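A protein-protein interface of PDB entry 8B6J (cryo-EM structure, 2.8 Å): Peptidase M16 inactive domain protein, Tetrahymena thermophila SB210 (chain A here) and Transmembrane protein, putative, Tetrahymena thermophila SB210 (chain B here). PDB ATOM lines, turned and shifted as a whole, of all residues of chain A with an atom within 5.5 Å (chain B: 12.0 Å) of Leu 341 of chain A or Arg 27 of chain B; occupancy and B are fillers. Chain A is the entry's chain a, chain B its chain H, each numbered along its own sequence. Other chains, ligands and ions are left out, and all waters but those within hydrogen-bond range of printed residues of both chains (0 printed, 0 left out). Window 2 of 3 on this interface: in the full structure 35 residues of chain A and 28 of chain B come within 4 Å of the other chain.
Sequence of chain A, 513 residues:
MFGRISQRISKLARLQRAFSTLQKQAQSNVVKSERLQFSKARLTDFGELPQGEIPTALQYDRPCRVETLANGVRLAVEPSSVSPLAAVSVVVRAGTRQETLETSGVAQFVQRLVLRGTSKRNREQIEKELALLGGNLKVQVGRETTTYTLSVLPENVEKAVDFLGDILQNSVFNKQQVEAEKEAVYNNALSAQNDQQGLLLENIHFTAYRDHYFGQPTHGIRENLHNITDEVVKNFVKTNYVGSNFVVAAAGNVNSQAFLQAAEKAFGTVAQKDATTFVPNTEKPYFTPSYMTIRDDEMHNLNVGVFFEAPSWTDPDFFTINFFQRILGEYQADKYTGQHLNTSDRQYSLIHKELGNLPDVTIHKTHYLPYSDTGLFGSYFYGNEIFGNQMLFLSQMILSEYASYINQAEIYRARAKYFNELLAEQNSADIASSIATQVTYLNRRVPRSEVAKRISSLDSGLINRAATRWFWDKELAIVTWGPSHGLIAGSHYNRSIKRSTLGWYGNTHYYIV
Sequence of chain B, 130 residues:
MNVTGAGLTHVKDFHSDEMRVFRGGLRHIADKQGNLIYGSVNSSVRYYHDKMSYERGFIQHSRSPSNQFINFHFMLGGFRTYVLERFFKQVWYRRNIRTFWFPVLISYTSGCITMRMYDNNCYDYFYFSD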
ATOM      1  N   TYR A 336       0.918 -18.915  -3.698  1.00  0.00           N
ATOM      2  CA  TYR A 336      -0.121 -19.344  -2.758  1.00  0.00           C
ATOM      3  C   TYR A 336      -1.324 -19.855  -3.557  1.00  0.00           C
ATOM      4  O   TYR A 336      -1.173 -20.349  -4.682  1.00  0.00           O
ATOM      5  CB  TYR A 336      -0.435 -18.208  -1.803  1.00  0.00           C
ATOM      6  CG  TYR A 336       0.753 -17.735  -1.001  1.00  0.00           C
ATOM      7  CD1 TYR A 336       1.201 -18.451   0.098  1.00  0.00           C
ATOM      8  CD2 TYR A 336       1.423 -16.568  -1.337  1.00  0.00           C
ATOM      9  CE1 TYR A 336       2.285 -18.023   0.836  1.00  0.00           C
ATOM     10  CE2 TYR A 336       2.507 -16.131  -0.605  1.00  0.00           C
ATOM     11  CZ  TYR A 336       2.933 -16.862   0.480  1.00  0.00           C
ATOM     12  OH  TYR A 336       4.013 -16.433   1.215  1.00  0.00           O
ATOM     13  N   THR A 337      -2.524 -19.730  -2.986  1.00  0.00           N
ATOM     14  CA  THR A 337      -3.721 -20.282  -3.610  1.00  0.00           C
ATOM     15  C   THR A 337      -4.008 -19.665  -4.971  1.00  0.00           C
ATOM     16  O   THR A 337      -4.729 -20.270  -5.772  1.00  0.00           O
ATOM     17  CB  THR A 337      -4.923 -20.077  -2.689  1.00  0.00           C
ATOM     18  OG1 THR A 337      -4.704 -20.780  -1.460  1.00  0.00           O
ATOM     19  CG2 THR A 337      -6.191 -20.590  -3.339  1.00  0.00           C
ATOM     20  N   GLY A 338      -3.468 -18.481  -5.253  1.00  0.00           N
ATOM     21  CA  GLY A 338      -3.719 -17.849  -6.535  1.00  0.00           C
ATOM     22  C   GLY A 338      -3.023 -18.521  -7.698  1.00  0.00           C
ATOM     23  O   GLY A 338      -3.375 -18.254  -8.851  1.00  0.00           O
ATOM     24  N   GLN A 339      -2.045 -19.384  -7.426  1.00  0.00           N
ATOM     25  CA  GLN A 339      -1.255 -19.997  -8.490  1.00  0.00           C
ATOM     26  C   GLN A 339      -1.185 -21.515  -8.414  1.00  0.00           C
ATOM     27  O   GLN A 339      -1.214 -22.171  -9.455  1.00  0.00           O
ATOM     28  CB  GLN A 339       0.167 -19.420  -8.467  1.00  0.00           C
ATOM     29  CG  GLN A 339       0.518 -18.599  -9.693  1.00  0.00           C
ATOM     30  CD  GLN A 339       0.550 -19.430 -10.957  1.00  0.00           C
ATOM     31  OE1 GLN A 339       0.504 -20.657 -10.904  1.00  0.00           O
ATOM     32  NE2 GLN A 339       0.628 -18.766 -12.101  1.00  0.00           N
ATOM     33  N   HIS A 340      -1.098 -22.092  -7.215  1.00  0.00           N
ATOM     34  CA  HIS A 340      -0.795 -23.517  -7.052  1.00  0.00           C
ATOM     35  C   HIS A 340      -1.883 -24.190  -6.221  1.00  0.00           C
ATOM     36  O   HIS A 340      -1.766 -24.280  -4.997  1.00  0.00           O
ATOM     37  CB  HIS A 340       0.577 -23.701  -6.406  1.00  0.00           C
ATOM     38  CG  HIS A 340       1.660 -22.896  -7.048  1.00  0.00           C
ATOM     39  ND1 HIS A 340       2.014 -23.044  -8.372  1.00  0.00           N
ATOM     40  CD2 HIS A 340       2.475 -21.938  -6.547  1.00  0.00           C
ATOM     41  CE1 HIS A 340       2.995 -22.209  -8.659  1.00  0.00           C
ATOM     42  NE2 HIS A 340       3.295 -21.526  -7.569  1.00  0.00           N
ATOM     43  N   LEU A 341      -2.935 -24.659  -6.885  1.00  0.00           N
ATOM     44  CA  LEU A 341      -3.924 -25.536  -6.267  1.00  0.00           C
ATOM     45  C   LEU A 341      -4.962 -25.901  -7.318  1.00  0.00           C
ATOM     46  O   LEU A 341      -5.123 -25.201  -8.321  1.00  0.00           O
ATOM     47  CB  LEU A 341      -4.599 -24.879  -5.060  1.00  0.00           C
ATOM     48  CG  LEU A 341      -4.189 -25.378  -3.672  1.00  0.00           C
ATOM     49  CD1 LEU A 341      -4.837 -24.516  -2.604  1.00  0.00           C
ATOM     50  CD2 LEU A 341      -4.562 -26.836  -3.481  1.00  0.00           C
ATOM     51  N   ASN A 342      -5.669 -27.007  -7.074  1.00  0.00           N
ATOM     52  CA  ASN A 342      -6.820 -27.336  -7.911  1.00  0.00           C
ATOM     53  C   ASN A 342      -8.004 -26.441  -7.581  1.00  0.00           C
ATOM     54  O   ASN A 342      -8.701 -25.962  -8.481  1.00  0.00           O
ATOM     55  CB  ASN A 342      -7.202 -28.807  -7.736  1.00  0.00           C
ATOM     56  CG  ASN A 342      -6.193 -29.749  -8.355  1.00  0.00           C
ATOM     57  OD1 ASN A 342      -5.024 -29.406  -8.518  1.00  0.00           O
ATOM     58  ND2 ASN A 342      -6.642 -30.947  -8.705  1.00  0.00           N
ATOM     59  N   THR A 343      -8.245 -26.205  -6.294  1.00  0.00           N
ATOM     60  CA  THR A 343      -9.300 -25.315  -5.840  1.00  0.00           C
ATOM     61  C   THR A 343      -8.823 -24.601  -4.586  1.00  0.00           C
ATOM     62  O   THR A 343      -7.988 -25.118  -3.841  1.00  0.00           O
ATOM     63  CB  THR A 343     -10.598 -26.077  -5.551  1.00  0.00           C
ATOM     64  OG1 THR A 343     -10.899 -26.945  -6.651  1.00  0.00           O
ATOM     65  CG2 THR A 343     -11.754 -25.112  -5.348  1.00  0.00           C
ATOM     66  N   SER A 344      -9.361 -23.401  -4.361  1.00  0.00           N
ATOM     67  CA  SER A 344      -8.971 -22.624  -3.192  1.00  0.00           C
ATOM     68  C   SER A 344      -9.380 -23.295  -1.887  1.00  0.00           C
ATOM     69  O   SER A 344      -8.774 -23.021  -0.848  1.00  0.00           O
ATOM     70  CB  SER A 344      -9.583 -21.227  -3.272  1.00  0.00           C
ATOM     71  OG  SER A 344      -9.151 -20.551  -4.439  1.00  0.00           O
ATOM     72  N   ARG A 346      -8.905 -26.309  -0.977  1.00  0.00           N
ATOM     73  CA  ARG A 346      -7.951 -27.331  -0.548  1.00  0.00           C
ATOM     74  C   ARG A 346      -6.704 -26.656   0.012  1.00  0.00           C
ATOM     75  O   ARG A 346      -5.664 -26.544  -0.639  1.00  0.00           O
ATOM     76  CB  ARG A 346      -7.611 -28.265  -1.702  1.00  0.00           C
ATOM     77  CG  ARG A 346      -8.716 -29.245  -2.047  1.00  0.00           C
ATOM     78  CD  ARG A 346      -9.685 -28.666  -3.056  1.00  0.00           C
ATOM     79  NE  ARG A 346     -10.937 -29.409  -3.093  1.00  0.00           N
ATOM     80  CZ  ARG A 346     -11.071 -30.619  -3.616  1.00  0.00           C
ATOM     81  NH1 ARG A 346     -10.045 -31.262  -4.146  1.00  0.00           N
ATOM     82  NH2 ARG A 346     -12.267 -31.201  -3.604  1.00  0.00           N
ATOM     83  N   GLN A 347      -6.819 -26.205   1.255  1.00  0.00           N
ATOM     84  CA  GLN A 347      -5.701 -25.621   1.986  1.00  0.00           C
ATOM     85  C   GLN A 347      -6.136 -25.472   3.438  1.00  0.00           C
ATOM     86  O   GLN A 347      -7.233 -25.885   3.822  1.00  0.00           O
ATOM     87  CB  GLN A 347      -5.271 -24.280   1.395  1.00  0.00           C
ATOM     88  CG  GLN A 347      -6.268 -23.156   1.622  1.00  0.00           C
ATOM     89  CD  GLN A 347      -5.827 -21.848   1.006  1.00  0.00           C
ATOM     90  OE1 GLN A 347      -6.646 -21.093   0.485  1.00  0.00           O
ATOM     91  NE2 GLN A 347      -4.530 -21.565   1.071  1.00  0.00           N
ATOM     92  N   ASP B  17     -15.806 -17.464 -19.223  1.00  0.00           N
ATOM     93  CA  ASP B  17     -15.460 -18.610 -18.394  1.00  0.00           C
ATOM     94  C   ASP B  17     -16.685 -19.274 -17.785  1.00  0.00           C
ATOM     95  O   ASP B  17     -16.555 -20.347 -17.188  1.00  0.00           O
ATOM     96  CB  ASP B  17     -14.493 -18.178 -17.292  1.00  0.00           C
ATOM     97  CG  ASP B  17     -13.206 -17.593 -17.846  1.00  0.00           C
ATOM     98  OD1 ASP B  17     -12.656 -18.170 -18.807  1.00  0.00           O
ATOM     99  OD2 ASP B  17     -12.751 -16.553 -17.328  1.00  0.00           O
ATOM    100  N   MET B  19     -20.066 -21.504 -17.856  1.00  0.00           N
ATOM    101  CA  MET B  19     -20.323 -22.791 -18.494  1.00  0.00           C
ATOM    102  C   MET B  19     -19.062 -23.637 -18.610  1.00  0.00           C
ATOM    103  O   MET B  19     -19.057 -24.631 -19.345  1.00  0.00           O
ATOM    104  CB  MET B  19     -20.955 -22.632 -19.881  1.00  0.00           C
ATOM    105  CG  MET B  19     -22.309 -21.945 -19.868  1.00  0.00           C
ATOM    106  SD  MET B  19     -23.083 -21.885 -21.493  1.00  0.00           S
ATOM    107  CE  MET B  19     -23.587 -23.588 -21.698  1.00  0.00           C
ATOM    108  N   ARG B  20     -17.993 -23.267 -17.911  1.00  0.00           N
ATOM    109  CA  ARG B  20     -16.773 -24.055 -17.840  1.00  0.00           C
ATOM    110  C   ARG B  20     -16.452 -24.351 -16.383  1.00  0.00           C
ATOM    111  O   ARG B  20     -16.779 -23.567 -15.489  1.00  0.00           O
ATOM    112  CB  ARG B  20     -15.589 -23.330 -18.489  1.00  0.00           C
ATOM    113  CG  ARG B  20     -15.566 -23.395 -20.003  1.00  0.00           C
ATOM    114  CD  ARG B  20     -14.198 -23.008 -20.541  1.00  0.00           C
ATOM    115  NE  ARG B  20     -14.059 -23.309 -21.962  1.00  0.00           N
ATOM    116  CZ  ARG B  20     -14.322 -22.459 -22.945  1.00  0.00           C
ATOM    117  NH1 ARG B  20     -14.749 -21.229 -22.704  1.00  0.00           N
ATOM    118  NH2 ARG B  20     -14.152 -22.852 -24.205  1.00  0.00           N
ATOM    119  N   VAL B  21     -15.812 -25.491 -16.151  1.00  0.00           N
ATOM    120  CA  VAL B  21     -15.436 -25.932 -14.815  1.00  0.00           C
ATOM    121  C   VAL B  21     -13.935 -25.792 -14.587  1.00  0.00           C
ATOM    122  O   VAL B  21     -13.502 -25.305 -13.544  1.00  0.00           O
ATOM    123  CB  VAL B  21     -15.898 -27.383 -14.562  1.00  0.00           C
ATOM    124  CG1 VAL B  21     -15.486 -27.835 -13.171  1.00  0.00           C
ATOM    125  CG2 VAL B  21     -17.400 -27.499 -14.740  1.00  0.00           C
ATOM    126  N   PHE B  22     -13.129 -26.213 -15.557  1.00  0.00           N
ATOM    127  CA  PHE B  22     -11.679 -26.227 -15.425  1.00  0.00           C
ATOM    128  C   PHE B  22     -11.059 -25.225 -16.389  1.00  0.00           C
ATOM    129  O   PHE B  22     -11.341 -25.259 -17.591  1.00  0.00           O
ATOM    130  CB  PHE B  22     -11.115 -27.622 -15.704  1.00  0.00           C
ATOM    131  CG  PHE B  22     -11.828 -28.723 -14.977  1.00  0.00           C
ATOM    132  CD1 PHE B  22     -11.582 -28.959 -13.638  1.00  0.00           C
ATOM    133  CD2 PHE B  22     -12.736 -29.527 -15.636  1.00  0.00           C
ATOM    134  CE1 PHE B  22     -12.234 -29.972 -12.969  1.00  0.00           C
ATOM    135  CE2 PHE B  22     -13.390 -30.541 -14.971  1.00  0.00           C
ATOM    136  CZ  PHE B  22     -13.138 -30.764 -13.637  1.00  0.00           C
ATOM    137  N   ARG B  23     -10.218 -24.336 -15.859  1.00  0.00           N
ATOM    138  CA  ARG B  23      -9.429 -23.460 -16.718  1.00  0.00           C
ATOM    139  C   ARG B  23      -8.245 -24.191 -17.332  1.00  0.00           C
ATOM    140  O   ARG B  23      -7.849 -23.883 -18.460  1.00  0.00           O
ATOM    141  CB  ARG B  23      -8.941 -22.232 -15.942  1.00  0.00           C
ATOM    142  CG  ARG B  23      -8.345 -22.521 -14.574  1.00  0.00           C
ATOM    143  CD  ARG B  23      -7.913 -21.237 -13.891  1.00  0.00           C
ATOM    144  NE  ARG B  23      -7.949 -21.354 -12.439  1.00  0.00           N
ATOM    145  CZ  ARG B  23      -7.702 -20.357 -11.600  1.00  0.00           C
ATOM    146  NH1 ARG B  23      -7.382 -19.150 -12.035  1.00  0.00           N
ATOM    147  NH2 ARG B  23      -7.782 -20.576 -10.291  1.00  0.00           N
ATOM    148  N   GLY B  24      -7.672 -25.151 -16.613  1.00  0.00           N
ATOM    149  CA  GLY B  24      -6.579 -25.942 -17.140  1.00  0.00           C
ATOM    150  C   GLY B  24      -6.448 -27.272 -16.429  1.00  0.00           C
ATOM    151  O   GLY B  24      -6.545 -27.332 -15.201  1.00  0.00           O
ATOM    152  N   GLY B  25      -6.228 -28.341 -17.185  1.00  0.00           N
ATOM    153  CA  GLY B  25      -6.100 -29.651 -16.568  1.00  0.00           C
ATOM    154  C   GLY B  25      -7.323 -29.966 -15.732  1.00  0.00           C
ATOM    155  O   GLY B  25      -8.464 -29.859 -16.190  1.00  0.00           O
ATOM    156  N   LEU B  26      -7.087 -30.363 -14.485  1.00  0.00           N
ATOM    157  CA  LEU B  26      -8.150 -30.608 -13.524  1.00  0.00           C
ATOM    158  C   LEU B  26      -8.358 -29.430 -12.583  1.00  0.00           C
ATOM    159  O   LEU B  26      -9.201 -29.508 -11.686  1.00  0.00           O
ATOM    160  CB  LEU B  26      -7.842 -31.872 -12.718  1.00  0.00           C
ATOM    161  CG  LEU B  26      -9.022 -32.578 -12.048  1.00  0.00           C
ATOM    162  CD1 LEU B  26      -9.981 -33.138 -13.086  1.00  0.00           C
ATOM    163  CD2 LEU B  26      -8.522 -33.679 -11.132  1.00  0.00           C
ATOM    164  N   ARG B  27      -7.610 -28.345 -12.768  1.00  0.00           N
ATOM    165  CA  ARG B  27      -7.752 -27.171 -11.921  1.00  0.00           C
ATOM    166  C   ARG B  27      -9.072 -26.466 -12.206  1.00  0.00           C
ATOM    167  O   ARG B  27      -9.514 -26.385 -13.354  1.00  0.00           O
ATOM    168  CB  ARG B  27      -6.583 -26.216 -12.156  1.00  0.00           C
ATOM    169  CG  ARG B  27      -6.570 -25.010 -11.240  1.00  0.00           C
ATOM    170  CD  ARG B  27      -5.428 -24.074 -11.584  1.00  0.00           C
ATOM    171  NE  ARG B  27      -5.361 -22.937 -10.675  1.00  0.00           N
ATOM    172  CZ  ARG B  27      -4.604 -21.865 -10.869  1.00  0.00           C
ATOM    173  NH1 ARG B  27      -3.842 -21.741 -11.943  1.00  0.00           N
ATOM    174  NH2 ARG B  27      -4.619 -20.890  -9.965  1.00  0.00           N
ATOM    175  N   HIS B  28      -9.695 -25.947 -11.155  1.00  0.00           N
ATOM    176  CA  HIS B  28     -10.988 -25.290 -11.271  1.00  0.00           C
ATOM    177  C   HIS B  28     -10.827 -23.805 -11.564  1.00  0.00           C
ATOM    178  O   HIS B  28      -9.809 -23.189 -11.237  1.00  0.00           O
ATOM    179  CB  HIS B  28     -11.800 -25.471  -9.990  1.00  0.00           C
ATOM    180  CG  HIS B  28     -12.424 -26.822  -9.861  1.00  0.00           C
ATOM    181  ND1 HIS B  28     -13.745 -27.061 -10.166  1.00  0.00           N
ATOM    182  CD2 HIS B  28     -11.908 -28.009  -9.467  1.00  0.00           C
ATOM    183  CE1 HIS B  28     -14.019 -28.336  -9.961  1.00  0.00           C
ATOM    184  NE2 HIS B  28     -12.921 -28.934  -9.538  1.00  0.00           N
ATOM    185  N   ILE B  29     -11.856 -23.233 -12.191  1.00  0.00           N
ATOM    186  CA  ILE B  29     -11.870 -21.801 -12.452  1.00  0.00           C
ATOM    187  C   ILE B  29     -12.152 -21.055 -11.154  1.00  0.00           C
ATOM    188  O   ILE B  29     -12.761 -21.592 -10.218  1.00  0.00           O
ATOM    189  CB  ILE B  29     -12.913 -21.456 -13.531  1.00  0.00           C
ATOM    190  CG1 ILE B  29     -12.581 -22.184 -14.835  1.00  0.00           C
ATOM    191  CG2 ILE B  29     -12.969 -19.954 -13.758  1.00  0.00           C
ATOM    192  CD1 ILE B  29     -13.624 -22.027 -15.919  1.00  0.00           C
ATOM    193  N   ALA B  30     -11.704 -19.804 -11.092  1.00  0.00           N
ATOM    194  CA  ALA B  30     -11.929 -18.997  -9.903  1.00  0.00           C
ATOM    195  C   ALA B  30     -13.421 -18.872  -9.629  1.00  0.00           C
ATOM    196  O   ALA B  30     -14.235 -18.782 -10.552  1.00  0.00           O
ATOM    197  CB  ALA B  30     -11.304 -17.615 -10.075  1.00  0.00           C
ATOM    198  N   ASP B  31     -13.779 -18.874  -8.345  1.00  0.00           N
ATOM    199  CA  ASP B  31     -15.190 -18.869  -7.973  1.00  0.00           C
ATOM    200  C   ASP B  31     -15.899 -17.629  -8.502  1.00  0.00           C
ATOM    201  O   ASP B  31     -17.037 -17.713  -8.977  1.00  0.00           O
ATOM    202  CB  ASP B  31     -15.326 -18.958  -6.454  1.00  0.00           C
ATOM    203  CG  ASP B  31     -16.767 -19.087  -6.004  1.00  0.00           C
ATOM    204  OD1 ASP B  31     -17.341 -20.185  -6.154  1.00  0.00           O
ATOM    205  OD2 ASP B  31     -17.325 -18.091  -5.498  1.00  0.00           O
ATOM    206  N   LYS B  32     -15.247 -16.471  -8.429  1.00  0.00           N
ATOM    207  CA  LYS B  32     -15.822 -15.201  -8.862  1.00  0.00           C
ATOM    208  C   LYS B  32     -15.191 -14.713 -10.163  1.00  0.00           C
ATOM    209  O   LYS B  32     -14.995 -13.514 -10.364  1.00  0.00           O
ATOM    210  CB  LYS B  32     -15.668 -14.145  -7.773  1.00  0.00           C
ATOM    211  CG  LYS B  32     -16.357 -14.493  -6.465  1.00  0.00           C
ATOM    212  CD  LYS B  32     -17.862 -14.608  -6.637  1.00  0.00           C
ATOM    213  CE  LYS B  32     -18.551 -14.890  -5.318  1.00  0.00           C
ATOM    214  NZ  LYS B  32     -18.329 -13.799  -4.331  1.00  0.00           N
ATOM    215  N   GLN B  33     -14.866 -15.640 -11.063  1.00  0.00           N
ATOM    216  CA  GLN B  33     -14.293 -15.246 -12.346  1.00  0.00           C
ATOM    217  C   GLN B  33     -15.285 -14.426 -13.161  1.00  0.00           C
ATOM    218  O   GLN B  33     -14.907 -13.443 -13.808  1.00  0.00           O
ATOM    219  CB  GLN B  33     -13.854 -16.487 -13.124  1.00  0.00           C
ATOM    220  CG  GLN B  33     -13.223 -16.193 -14.476  1.00  0.00           C
ATOM    221  CD  GLN B  33     -11.930 -15.415 -14.362  1.00  0.00           C
ATOM    222  OE1 GLN B  33     -11.345 -15.315 -13.286  1.00  0.00           O
ATOM    223  NE2 GLN B  33     -11.475 -14.860 -15.478  1.00  0.00           N
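Among the printed residues, merely in contact across the chains: Gln 339 of chain A with Arg 27 of chain B (3.6 Å), Asn 342 of chain A with Arg 27 of chain B (3.6 Å) and Thr 343 of chain A with His 28 of chain B (3.2 Å).
O of Gly 338 of chain A is in hydrogen-bond range of NH2 of Arg 27 of chain B, 3.1 Å away. The backbone carbonyl oxygen (O) of Leu 341 of chain A lies close to the guanidinium group (NE) of Arg 27 of chain B, at 3.3 Å. N of His 28 of chain B is in hydrogen-bond range of O of Asn 342 of chain A, 2.9 Å away.
Among the printed residues, no Asp or Glu carboxylate lies within 4 Å of a Lys or Arg side-chain nitrogen of the other chain.
Leu 341 of chain A touches just one residue of chain B: Arg 27. Arg 27 of chain B touches just these residues of chain A: Gly 338 (3.1 Å), Gln 339 (3.6 Å), Leu 341 (3.3 Å) and Asn 342 (3.6 Å). Thr 337 of chain A touches none of the printed residues of chain B. Gly 338 of chain A touches just one residue of chain B: Arg 27. His 340 of chain A touches none of the printed residues of chain B. Asn 342 of chain A touches just these residues of chain B: Arg 27 and His 28. Thr 343 of chain A touches one residue of chain B. Printed residues of chain A within 4 Å of His 28 of chain B: Asn 342 and Thr 343. Arg 346 of chain A touches none of the printed residues of chain B. Gly 25 of chain B touches none of the printed residues of chain A. The nearest residue of chain B that does not touch Leu 341 of chain A is His 28 of chain B (5.4 Å). The nearest residue of chain A that does not touch Arg 27 of chain B is Thr 337 of chain A (4.2 Å).
The guanidinium group of Arg 23 of chain B lies within hydrogen-bond range of the backbone carbonyl oxygen of His 28 of chain B, at 2.9 Å.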
